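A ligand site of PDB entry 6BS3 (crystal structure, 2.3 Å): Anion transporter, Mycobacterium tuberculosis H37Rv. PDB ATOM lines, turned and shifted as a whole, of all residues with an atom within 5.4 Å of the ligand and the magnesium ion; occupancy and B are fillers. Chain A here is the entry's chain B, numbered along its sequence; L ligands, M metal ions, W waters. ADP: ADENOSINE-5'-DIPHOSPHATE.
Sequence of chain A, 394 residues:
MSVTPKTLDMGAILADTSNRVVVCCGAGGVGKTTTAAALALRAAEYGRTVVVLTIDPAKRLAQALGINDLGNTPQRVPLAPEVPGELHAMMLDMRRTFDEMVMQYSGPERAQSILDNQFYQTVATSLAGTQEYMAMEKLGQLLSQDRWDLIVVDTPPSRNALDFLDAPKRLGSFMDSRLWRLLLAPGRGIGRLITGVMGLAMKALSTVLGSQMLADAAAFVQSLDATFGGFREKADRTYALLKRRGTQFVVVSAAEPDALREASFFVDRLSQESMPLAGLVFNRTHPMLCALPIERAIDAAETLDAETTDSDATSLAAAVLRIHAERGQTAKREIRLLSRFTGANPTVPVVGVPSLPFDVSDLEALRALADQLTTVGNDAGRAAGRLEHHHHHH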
ATOM      1  N   ALA A  27      -1.444  -8.897   0.539  1.00  0.00           N
ATOM      2  CA  ALA A  27      -1.956  -9.670   1.668  1.00  0.00           C
ATOM      3  C   ALA A  27      -0.818  -9.765   2.715  1.00  0.00           C
ATOM      4  O   ALA A  27       0.314  -9.431   2.411  1.00  0.00           O
ATOM      5  CB  ALA A  27      -2.364 -11.065   1.205  1.00  0.00           C
ATOM      6  N   GLY A  28      -1.138 -10.170   3.933  1.00  0.00           N
ATOM      7  CA  GLY A  28      -0.138 -10.348   4.975  1.00  0.00           C
ATOM      8  C   GLY A  28       0.615 -11.654   4.787  1.00  0.00           C
ATOM      9  O   GLY A  28       0.072 -12.600   4.205  1.00  0.00           O
ATOM     10  N   GLY A  29       1.833 -11.731   5.289  1.00  0.00           N
ATOM     11  CA  GLY A  29       2.686 -12.917   5.216  1.00  0.00           C
ATOM     12  C   GLY A  29       3.379 -13.147   3.884  1.00  0.00           C
ATOM     13  O   GLY A  29       3.891 -14.256   3.662  1.00  0.00           O
ATOM     14  N   VAL A  30       3.439 -12.137   3.002  1.00  0.00           N
ATOM     15  CA  VAL A  30       4.037 -12.283   1.667  1.00  0.00           C
ATOM     16  C   VAL A  30       5.476 -11.714   1.552  1.00  0.00           C
ATOM     17  O   VAL A  30       6.172 -12.045   0.587  1.00  0.00           O
ATOM     18  CB  VAL A  30       3.127 -11.698   0.560  1.00  0.00           C
ATOM     19  CG1 VAL A  30       1.764 -12.390   0.545  1.00  0.00           C
ATOM     20  CG2 VAL A  30       2.976 -10.180   0.689  1.00  0.00           C
ATOM     21  N   GLY A  31       5.878 -10.858   2.487  1.00  0.00           N
ATOM     22  CA  GLY A  31       7.153 -10.168   2.468  1.00  0.00           C
ATOM     23  C   GLY A  31       7.023  -8.652   2.302  1.00  0.00           C
ATOM     24  O   GLY A  31       7.973  -8.021   1.844  1.00  0.00           O
ATOM     25  N   LYS A  32       5.890  -8.042   2.719  1.00  0.00           N
ATOM     26  CA  LYS A  32       5.726  -6.581   2.622  1.00  0.00           C
ATOM     27  C   LYS A  32       6.726  -5.807   3.470  1.00  0.00           C
ATOM     28  O   LYS A  32       7.330  -4.874   2.948  1.00  0.00           O
ATOM     29  CB  LYS A  32       4.289  -6.119   2.955  1.00  0.00           C
ATOM     30  CG  LYS A  32       3.185  -6.701   2.094  1.00  0.00           C
ATOM     31  CD  LYS A  32       1.886  -5.948   2.284  1.00  0.00           C
ATOM     32  CE  LYS A  32       1.127  -6.220   3.558  1.00  0.00           C
ATOM     33  NZ  LYS A  32      -0.122  -5.408   3.639  1.00  0.00           N
ATOM     34  N   THR A  33       6.877  -6.150   4.762  1.00  0.00           N
ATOM     35  CA  THR A  33       7.779  -5.428   5.698  1.00  0.00           C
ATOM     36  C   THR A  33       9.222  -5.490   5.278  1.00  0.00           C
ATOM     37  O   THR A  33       9.865  -4.446   5.242  1.00  0.00           O
ATOM     38  CB  THR A  33       7.590  -5.883   7.155  1.00  0.00           C
ATOM     39  OG1 THR A  33       6.244  -5.638   7.495  1.00  0.00           O
ATOM     40  CG2 THR A  33       8.490  -5.118   8.150  1.00  0.00           C
ATOM     41  N   THR A  34       9.736  -6.700   5.003  1.00  0.00           N
ATOM     42  CA  THR A  34      11.114  -6.956   4.553  1.00  0.00           C
ATOM     43  C   THR A  34      11.373  -6.293   3.201  1.00  0.00           C
ATOM     44  O   THR A  34      12.445  -5.751   3.028  1.00  0.00           O
ATOM     45  CB  THR A  34      11.417  -8.464   4.543  1.00  0.00           C
ATOM     46  OG1 THR A  34      10.426  -9.119   3.759  1.00  0.00           O
ATOM     47  CG2 THR A  34      11.443  -9.072   5.931  1.00  0.00           C
ATOM     48  N   THR A  35      10.404  -6.344   2.253  1.00  0.00           N
ATOM     49  CA  THR A  35      10.521  -5.669   0.938  1.00  0.00           C
ATOM     50  C   THR A  35      10.624  -4.163   1.172  1.00  0.00           C
ATOM     51  O   THR A  35      11.514  -3.532   0.606  1.00  0.00           O
ATOM     52  CB  THR A  35       9.329  -6.046   0.001  1.00  0.00           C
ATOM     53  OG1 THR A  35       9.418  -7.425  -0.304  1.00  0.00           O
ATOM     54  CG2 THR A  35       9.305  -5.242  -1.303  1.00  0.00           C
ATOM     55  N   ILE A  55       5.401  -1.499   9.783  1.00  0.00           N
ATOM     56  CA  ILE A  55       4.234  -1.787  10.614  1.00  0.00           C
ATOM     57  C   ILE A  55       4.604  -2.813  11.672  1.00  0.00           C
ATOM     58  O   ILE A  55       4.592  -2.510  12.866  1.00  0.00           O
ATOM     59  CB  ILE A  55       2.980  -2.213   9.781  1.00  0.00           C
ATOM     60  CG1 ILE A  55       2.602  -1.159   8.706  1.00  0.00           C
ATOM     61  CG2 ILE A  55       1.771  -2.558  10.710  1.00  0.00           C
ATOM     62  CD1 ILE A  55       2.287   0.322   9.184  1.00  0.00           C
ATOM     63  N   ASP A  56       4.942  -4.010  11.215  1.00  0.00           N
ATOM     64  CA  ASP A  56       5.206  -5.150  12.077  1.00  0.00           C
ATOM     65  C   ASP A  56       6.484  -5.912  11.725  1.00  0.00           C
ATOM     66  O   ASP A  56       6.403  -7.094  11.357  1.00  0.00           O
ATOM     67  CB  ASP A  56       3.961  -6.088  12.057  1.00  0.00           C
ATOM     68  CG  ASP A  56       3.523  -6.563  10.660  1.00  0.00           C
ATOM     69  OD1 ASP A  56       4.056  -6.029   9.642  1.00  0.00           O
ATOM     70  OD2 ASP A  56       2.662  -7.482  10.587  1.00  0.00           O
ATOM     71  N   ALA A  58       9.605  -8.327  12.356  1.00  0.00           N
ATOM     72  CA  ALA A  58       9.901  -9.408  13.293  1.00  0.00           C
ATOM     73  C   ALA A  58      10.971  -8.852  14.247  1.00  0.00           C
ATOM     74  O   ALA A  58      11.760  -8.002  13.830  1.00  0.00           O
ATOM     75  CB  ALA A  58      10.451 -10.606  12.538  1.00  0.00           C
ATOM     76  N   ASP A 154       5.256   0.662   4.545  1.00  0.00           N
ATOM     77  CA  ASP A 154       4.811  -0.705   4.758  1.00  0.00           C
ATOM     78  C   ASP A 154       3.296  -0.602   5.104  1.00  0.00           C
ATOM     79  O   ASP A 154       2.829   0.463   5.544  1.00  0.00           O
ATOM     80  CB  ASP A 154       5.640  -1.320   5.883  1.00  0.00           C
ATOM     81  CG  ASP A 154       5.318  -2.737   6.261  1.00  0.00           C
ATOM     82  OD1 ASP A 154       4.683  -3.454   5.441  1.00  0.00           O
ATOM     83  OD2 ASP A 154       5.706  -3.136   7.380  1.00  0.00           O
ATOM     84  N   THR A 155       2.516  -1.642   4.820  1.00  0.00           N
ATOM     85  CA  THR A 155       1.077  -1.604   5.065  1.00  0.00           C
ATOM     86  C   THR A 155       0.656  -2.744   5.992  1.00  0.00           C
ATOM     87  O   THR A 155       1.269  -3.813   5.913  1.00  0.00           O
ATOM     88  CB  THR A 155       0.274  -1.551   3.758  1.00  0.00           C
ATOM     89  OG1 THR A 155       0.496  -2.744   3.003  1.00  0.00           O
ATOM     90  CG2 THR A 155       0.561  -0.318   2.934  1.00  0.00           C
ATOM     91  N   PRO A 157      -0.832  -6.106   7.863  1.00  0.00           N
ATOM     92  CA  PRO A 157      -1.249  -7.384   7.297  1.00  0.00           C
ATOM     93  C   PRO A 157      -2.776  -7.527   7.311  1.00  0.00           C
ATOM     94  O   PRO A 157      -3.447  -7.004   8.185  1.00  0.00           O
ATOM     95  CB  PRO A 157      -0.601  -8.405   8.246  1.00  0.00           C
ATOM     96  CG  PRO A 157      -0.580  -7.698   9.562  1.00  0.00           C
ATOM     97  CD  PRO A 157      -0.181  -6.296   9.171  1.00  0.00           C
ATOM     98  N   ASN A 283       7.365 -12.867  -4.673  1.00  0.00           N
ATOM     99  CA  ASN A 283       8.289 -13.307  -3.639  1.00  0.00           C
ATOM    100  C   ASN A 283       8.216 -14.801  -3.302  1.00  0.00           C
ATOM    101  O   ASN A 283       7.167 -15.426  -3.448  1.00  0.00           O
ATOM    102  CB  ASN A 283       8.078 -12.450  -2.387  1.00  0.00           C
ATOM    103  CG  ASN A 283       9.231 -12.452  -1.414  1.00  0.00           C
ATOM    104  OD1 ASN A 283      10.390 -12.630  -1.778  1.00  0.00           O
ATOM    105  ND2 ASN A 283       8.929 -12.259  -0.141  1.00  0.00           N
ATOM    106  N   ARG A 284       9.347 -15.357  -2.799  1.00  0.00           N
ATOM    107  CA  ARG A 284       9.540 -16.736  -2.332  1.00  0.00           C
ATOM    108  C   ARG A 284       9.499 -17.760  -3.449  1.00  0.00           C
ATOM    109  O   ARG A 284       8.879 -18.815  -3.280  1.00  0.00           O
ATOM    110  CB  ARG A 284       8.540 -17.138  -1.199  1.00  0.00           C
ATOM    111  CG  ARG A 284       8.324 -16.148  -0.061  1.00  0.00           C
ATOM    112  CD  ARG A 284       9.597 -15.781   0.661  1.00  0.00           C
ATOM    113  NE  ARG A 284      10.150 -16.899   1.443  1.00  0.00           N
ATOM    114  CZ  ARG A 284       9.860 -17.136   2.716  1.00  0.00           C
ATOM    115  NH1 ARG A 284       8.994 -16.361   3.366  1.00  0.00           N
ATOM    116  NH2 ARG A 284      10.412 -18.162   3.343  1.00  0.00           N
ATOM    117  N   VAL A 353      11.352 -12.887  -6.904  1.00  0.00           N
ATOM    118  CA  VAL A 353      12.317 -12.891  -5.807  1.00  0.00           C
ATOM    119  C   VAL A 353      12.427 -14.317  -5.241  1.00  0.00           C
ATOM    120  O   VAL A 353      11.464 -14.816  -4.654  1.00  0.00           O
ATOM    121  CB  VAL A 353      11.917 -11.909  -4.688  1.00  0.00           C
ATOM    122  CG1 VAL A 353      12.864 -12.044  -3.500  1.00  0.00           C
ATOM    123  CG2 VAL A 353      11.909 -10.484  -5.204  1.00  0.00           C
ATOM    124  N   PRO A 354      13.601 -14.966  -5.381  1.00  0.00           N
ATOM    125  CA  PRO A 354      13.751 -16.322  -4.826  1.00  0.00           C
ATOM    126  C   PRO A 354      13.719 -16.376  -3.296  1.00  0.00           C
ATOM    127  O   PRO A 354      14.038 -15.399  -2.606  1.00  0.00           O
ATOM    128  CB  PRO A 354      15.107 -16.795  -5.377  1.00  0.00           C
ATOM    129  CG  PRO A 354      15.457 -15.803  -6.484  1.00  0.00           C
ATOM    130  CD  PRO A 354      14.843 -14.514  -6.043  1.00  0.00           C
ATOM    131  N   SER A 355      13.313 -17.533  -2.775  1.00  0.00           N
ATOM    132  CA  SER A 355      13.305 -17.798  -1.340  1.00  0.00           C
ATOM    133  C   SER A 355      14.782 -17.911  -0.941  1.00  0.00           C
ATOM    134  O   SER A 355      15.506 -18.705  -1.526  1.00  0.00           O
ATOM    135  CB  SER A 355      12.547 -19.085  -1.051  1.00  0.00           C
ATOM    136  OG  SER A 355      12.304 -19.179   0.332  1.00  0.00           O
ATOM    137  N   LEU A 356      15.241 -17.002  -0.070  1.00  0.00           N
ATOM    138  CA  LEU A 356      16.643 -16.931   0.368  1.00  0.00           C
ATOM    139  C   LEU A 356      16.908 -17.972   1.457  1.00  0.00           C
ATOM    140  O   LEU A 356      16.034 -18.172   2.301  1.00  0.00           O
ATOM    141  CB  LEU A 356      17.051 -15.506   0.804  1.00  0.00           C
ATOM    142  CG  LEU A 356      16.860 -14.379  -0.245  1.00  0.00           C
ATOM    143  CD1 LEU A 356      16.963 -13.020   0.397  1.00  0.00           C
ATOM    144  CD2 LEU A 356      17.878 -14.471  -1.396  1.00  0.00           C
ATOM    145  N   PHE A 358      18.087 -18.232   4.343  1.00  0.00           N
ATOM    146  CA  PHE A 358      18.333 -17.617   5.658  1.00  0.00           C
ATOM    147  C   PHE A 358      17.162 -16.692   5.959  1.00  0.00           C
ATOM    148  O   PHE A 358      16.438 -16.309   5.036  1.00  0.00           O
ATOM    149  CB  PHE A 358      19.662 -16.802   5.658  1.00  0.00           C
ATOM    150  CG  PHE A 358      19.870 -15.899   4.467  1.00  0.00           C
ATOM    151  CD1 PHE A 358      19.241 -14.655   4.381  1.00  0.00           C
ATOM    152  CD2 PHE A 358      20.730 -16.272   3.429  1.00  0.00           C
ATOM    153  CE1 PHE A 358      19.456 -13.818   3.292  1.00  0.00           C
ATOM    154  CE2 PHE A 358      20.954 -15.433   2.346  1.00  0.00           C
ATOM    155  CZ  PHE A 358      20.313 -14.208   2.283  1.00  0.00           C
ATOM    156  N   ASP A 359      17.011 -16.311   7.232  1.00  0.00           N
ATOM    157  CA  ASP A 359      15.939 -15.405   7.628  1.00  0.00           C
ATOM    158  C   ASP A 359      16.278 -13.954   7.268  1.00  0.00           C
ATOM    159  O   ASP A 359      17.436 -13.555   7.380  1.00  0.00           O
ATOM    160  CB  ASP A 359      15.625 -15.558   9.133  1.00  0.00           C
ATOM    161  CG  ASP A 359      14.290 -14.937   9.547  1.00  0.00           C
ATOM    162  OD1 ASP A 359      14.265 -14.216  10.551  1.00  0.00           O
ATOM    163  OD2 ASP A 359      13.274 -15.190   8.845  1.00  0.00           O
ATOM    164  N   VAL A 360      15.295 -13.167   6.789  1.00  0.00           N
ATOM    165  CA  VAL A 360      15.563 -11.765   6.441  1.00  0.00           C
ATOM    166  C   VAL A 360      15.362 -10.899   7.693  1.00  0.00           C
ATOM    167  O   VAL A 360      14.350 -10.191   7.832  1.00  0.00           O
ATOM    168  CB  VAL A 360      14.832 -11.267   5.168  1.00  0.00           C
ATOM    169  CG1 VAL A 360      15.398  -9.921   4.721  1.00  0.00           C
ATOM    170  CG2 VAL A 360      14.930 -12.289   4.031  1.00  0.00           C
ATOM    171  N   SER A 361      16.322 -10.997   8.639  1.00  0.00           N
ATOM    172  CA  SER A 361      16.238 -10.356   9.932  1.00  0.00           C
ATOM    173  C   SER A 361      17.487  -9.550  10.384  1.00  0.00           C
ATOM    174  O   SER A 361      17.589  -9.200  11.559  1.00  0.00           O
ATOM    175  CB  SER A 361      15.854 -11.393  10.998  1.00  0.00           C
ATOM    176  OG  SER A 361      16.625 -12.579  10.897  1.00  0.00           O
ATOM    177  N   LEU A 369      18.430  -9.347  -0.095  1.00  0.00           N
ATOM    178  CA  LEU A 369      17.061  -9.231  -0.611  1.00  0.00           C
ATOM    179  C   LEU A 369      16.965  -8.078  -1.626  1.00  0.00           C
ATOM    180  O   LEU A 369      16.421  -8.280  -2.711  1.00  0.00           O
ATOM    181  CB  LEU A 369      16.030  -9.047   0.542  1.00  0.00           C
ATOM    182  CG  LEU A 369      14.544  -9.025   0.153  1.00  0.00           C
ATOM    183  CD1 LEU A 369      14.127 -10.361  -0.443  1.00  0.00           C
ATOM    184  CD2 LEU A 369      13.675  -8.701   1.346  1.00  0.00           C
HETATM  185  PB  ADP L   1       4.657  -9.469   5.705  1.00  0.00           P
HETATM  186  O1B ADP L   1       4.121  -9.560   4.304  1.00  0.00           O
HETATM  187  O2B ADP L   1       4.858  -8.058   6.173  1.00  0.00           O
HETATM  188  O3B ADP L   1       3.761 -10.212   6.623  1.00  0.00           O
HETATM  189  PA  ADP L   1       7.472 -10.154   6.251  1.00  0.00           P
HETATM  190  O1A ADP L   1       8.209  -9.105   5.445  1.00  0.00           O
HETATM  191  O2A ADP L   1       7.375  -9.806   7.690  1.00  0.00           O
HETATM  192  O3A ADP L   1       6.002 -10.306   5.657  1.00  0.00           O
HETATM  193  O5' ADP L   1       8.044 -11.551   5.857  1.00  0.00           O
HETATM  194  C5' ADP L   1       7.508 -12.788   6.379  1.00  0.00           C
HETATM  195  C4' ADP L   1       8.656 -13.737   6.616  1.00  0.00           C
HETATM  196  O4' ADP L   1       9.213 -14.131   5.341  1.00  0.00           O
HETATM  197  C3' ADP L   1       9.813 -13.177   7.447  1.00  0.00           C
HETATM  198  O3' ADP L   1      10.218 -14.040   8.501  1.00  0.00           O
HETATM  199  C2' ADP L   1      10.892 -12.873   6.398  1.00  0.00           C
HETATM  200  O2' ADP L   1      12.197 -12.985   6.934  1.00  0.00           O
HETATM  201  C1' ADP L   1      10.614 -13.941   5.348  1.00  0.00           C
HETATM  202  N9  ADP L   1      11.039 -13.570   3.995  1.00  0.00           N
HETATM  203  C8  ADP L   1      10.532 -12.557   3.222  1.00  0.00           C
HETATM  204  N7  ADP L   1      10.985 -12.540   1.995  1.00  0.00           N
HETATM  205  C5  ADP L   1      11.861 -13.610   1.952  1.00  0.00           C
HETATM  206  C6  ADP L   1      12.656 -14.148   0.908  1.00  0.00           C
HETATM  207  N6  ADP L   1      12.638 -13.688  -0.350  1.00  0.00           N
HETATM  208  N1  ADP L   1      13.448 -15.204   1.207  1.00  0.00           N
HETATM  209  C2  ADP L   1      13.438 -15.687   2.459  1.00  0.00           C
HETATM  210  N3  ADP L   1      12.726 -15.280   3.506  1.00  0.00           N
HETATM  211  C4  ADP L   1      11.929 -14.240   3.183  1.00  0.00           C
HETATM  212 MG    MG M   1       4.457  -6.915   7.727  1.00  0.00          MG
HETATM  213  O   HOH W   1      12.061 -10.514   9.213  1.00  0.00           O
HETATM  214  O   HOH W   2       5.733  -8.217   9.025  1.00  0.00           O
HETATM  215  O   HOH W   3       8.227 -13.910  10.444  1.00  0.00           O
HETATM  216  O   HOH W   4       2.777  -8.178   8.016  1.00  0.00           O
HETATM  217  O   HOH W   5       3.397  -5.419   6.654  1.00  0.00           O
HETATM  218  O   HOH W   6      11.866 -12.897  10.492  1.00  0.00           O
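O2B of the ligand is bound to the magnesium ion, 2.0 Å away. The magnesium ion is bound by water W4 (2.1 Å). Water W5 is bound to the magnesium ion (2.1 Å). OD1 of Asp 56 is bound to the magnesium ion (2.1 Å). The side-chain hydroxyl (OG1) of Thr 33 binds the magnesium ion, at 2.2 Å. Water W2 is bound to the magnesium ion. The magnesium ion has six donor atoms within binding distance.
Asp 154 touches the magnesium ion. The nearest printed residue that does not touch the magnesium ion is Thr 155 (4.8 Å).
Gly 28 touches the ligand. Val 353 touches the ligand. CA of Ser 355 touches N1 of the ligand, at 3.6 Å. Leu 369 touches the ligand (CD1 to N6, 3.6 Å). Hydrophobic or aromatic side chains that line the ligand: Val 30, Val 353, Leu 356, Val 360 and Leu 369. 16 residues have an atom within 4 Å of the ligand: Gly 28, Gly 29, Val 30, Gly 31, Lys 32, Thr 33, Thr 34, Asn 283, Arg 284, Val 353, Pro 354, Ser 355, Leu 356, Asp 359, Val 360 and Leu 369. The nearest printed residue that does not touch the ligand is Phe 358 (4.003 Å).
Water W5 lies within hydrogen-bond range of the side-chain carboxylate (OD1) of Asp 154 and the backbone carbonyl oxygen (O) of Thr 155. Water W4 bridges O3B of the ligand (2.7 Å) and OD2 of Asp 56 (2.7 Å). Water W2 lies within hydrogen-bond range of O2A of the ligand and O of Asp 56. Water W6 bridges OD1 of Asp 359 (2.7 Å) and O3' of the ligand (2.8 Å). Water W1 lies within hydrogen-bond range of O of Val 360 (2.7 Å) and O2' of the ligand (3.4 Å).
O1A of the ligand is in hydrogen-bond range of N of Thr 33. The backbone NH (N) of Thr 34 sits at hydrogen-bond distance from an oxygen (O1A) of the ligand (2.9 Å). An oxygen (O1A) of the ligand is in hydrogen-bond range of the side-chain hydroxyl of Thr 34, 2.8 Å away. The backbone NH (N) of Gly 29 sits at hydrogen-bond distance from an oxygen (O3B) of the ligand (2.8 Å). N of Lys 32 sits at hydrogen-bond distance from O1B of the ligand. The backbone NH (N) of Gly 31 is in hydrogen-bond range of an oxygen (O1B) of the ligand (2.8 Å). N1 of the ligand is in hydrogen-bond range of N of Leu 356. The side-chain amide oxygen (OD1) of Asn 283 lies within hydrogen-bond range of a nitrogen (N6) of the ligand (2.9 Å). O1B of the ligand lies within hydrogen-bond range of N of Val 30 (3.0 Å). NH1 of Arg 284 lies within hydrogen-bond range of O4' of the ligand (3.0 Å). N of Val 360 sits at hydrogen-bond distance from O2' of the ligand (3.1 Å). OD2 of Asp 359 is in hydrogen-bond range of O2' of the ligand (3.1 Å). O of Pro 354 is in hydrogen-bond range of N6 of the ligand.
The side-chain hydroxyl of Thr 33 lies close to the side-chain carboxylate of Asp 154, 2.6 Å away. The side-chain hydroxyl (OG1) of Thr 34 is in hydrogen-bond range of the backbone carbonyl oxygen (O) of Gly 31, at 3.3 Å. NZ of Lys 32 lies within hydrogen-bond range of OG1 of Thr 155 (2.8 Å). The side-chain amide nitrogen (ND2) of Asn 283 sits at hydrogen-bond distance from the backbone carbonyl oxygen (O) of Val 30 (2.9 Å). The backbone carbonyl oxygen of Val 353 sits at hydrogen-bond distance from the backbone NH of Arg 284, at 2.9 Å. NE of Arg 284 sits at hydrogen-bond distance from OG of Ser 355, at 3.3 Å. The side-chain carboxylate (OD1) of Asp 359 lies within hydrogen-bond range of the side-chain hydroxyl (OG) of Ser 361 (2.9 Å). OD2 of Asp 154 lies within hydrogen-bond range of N of Ile 55.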
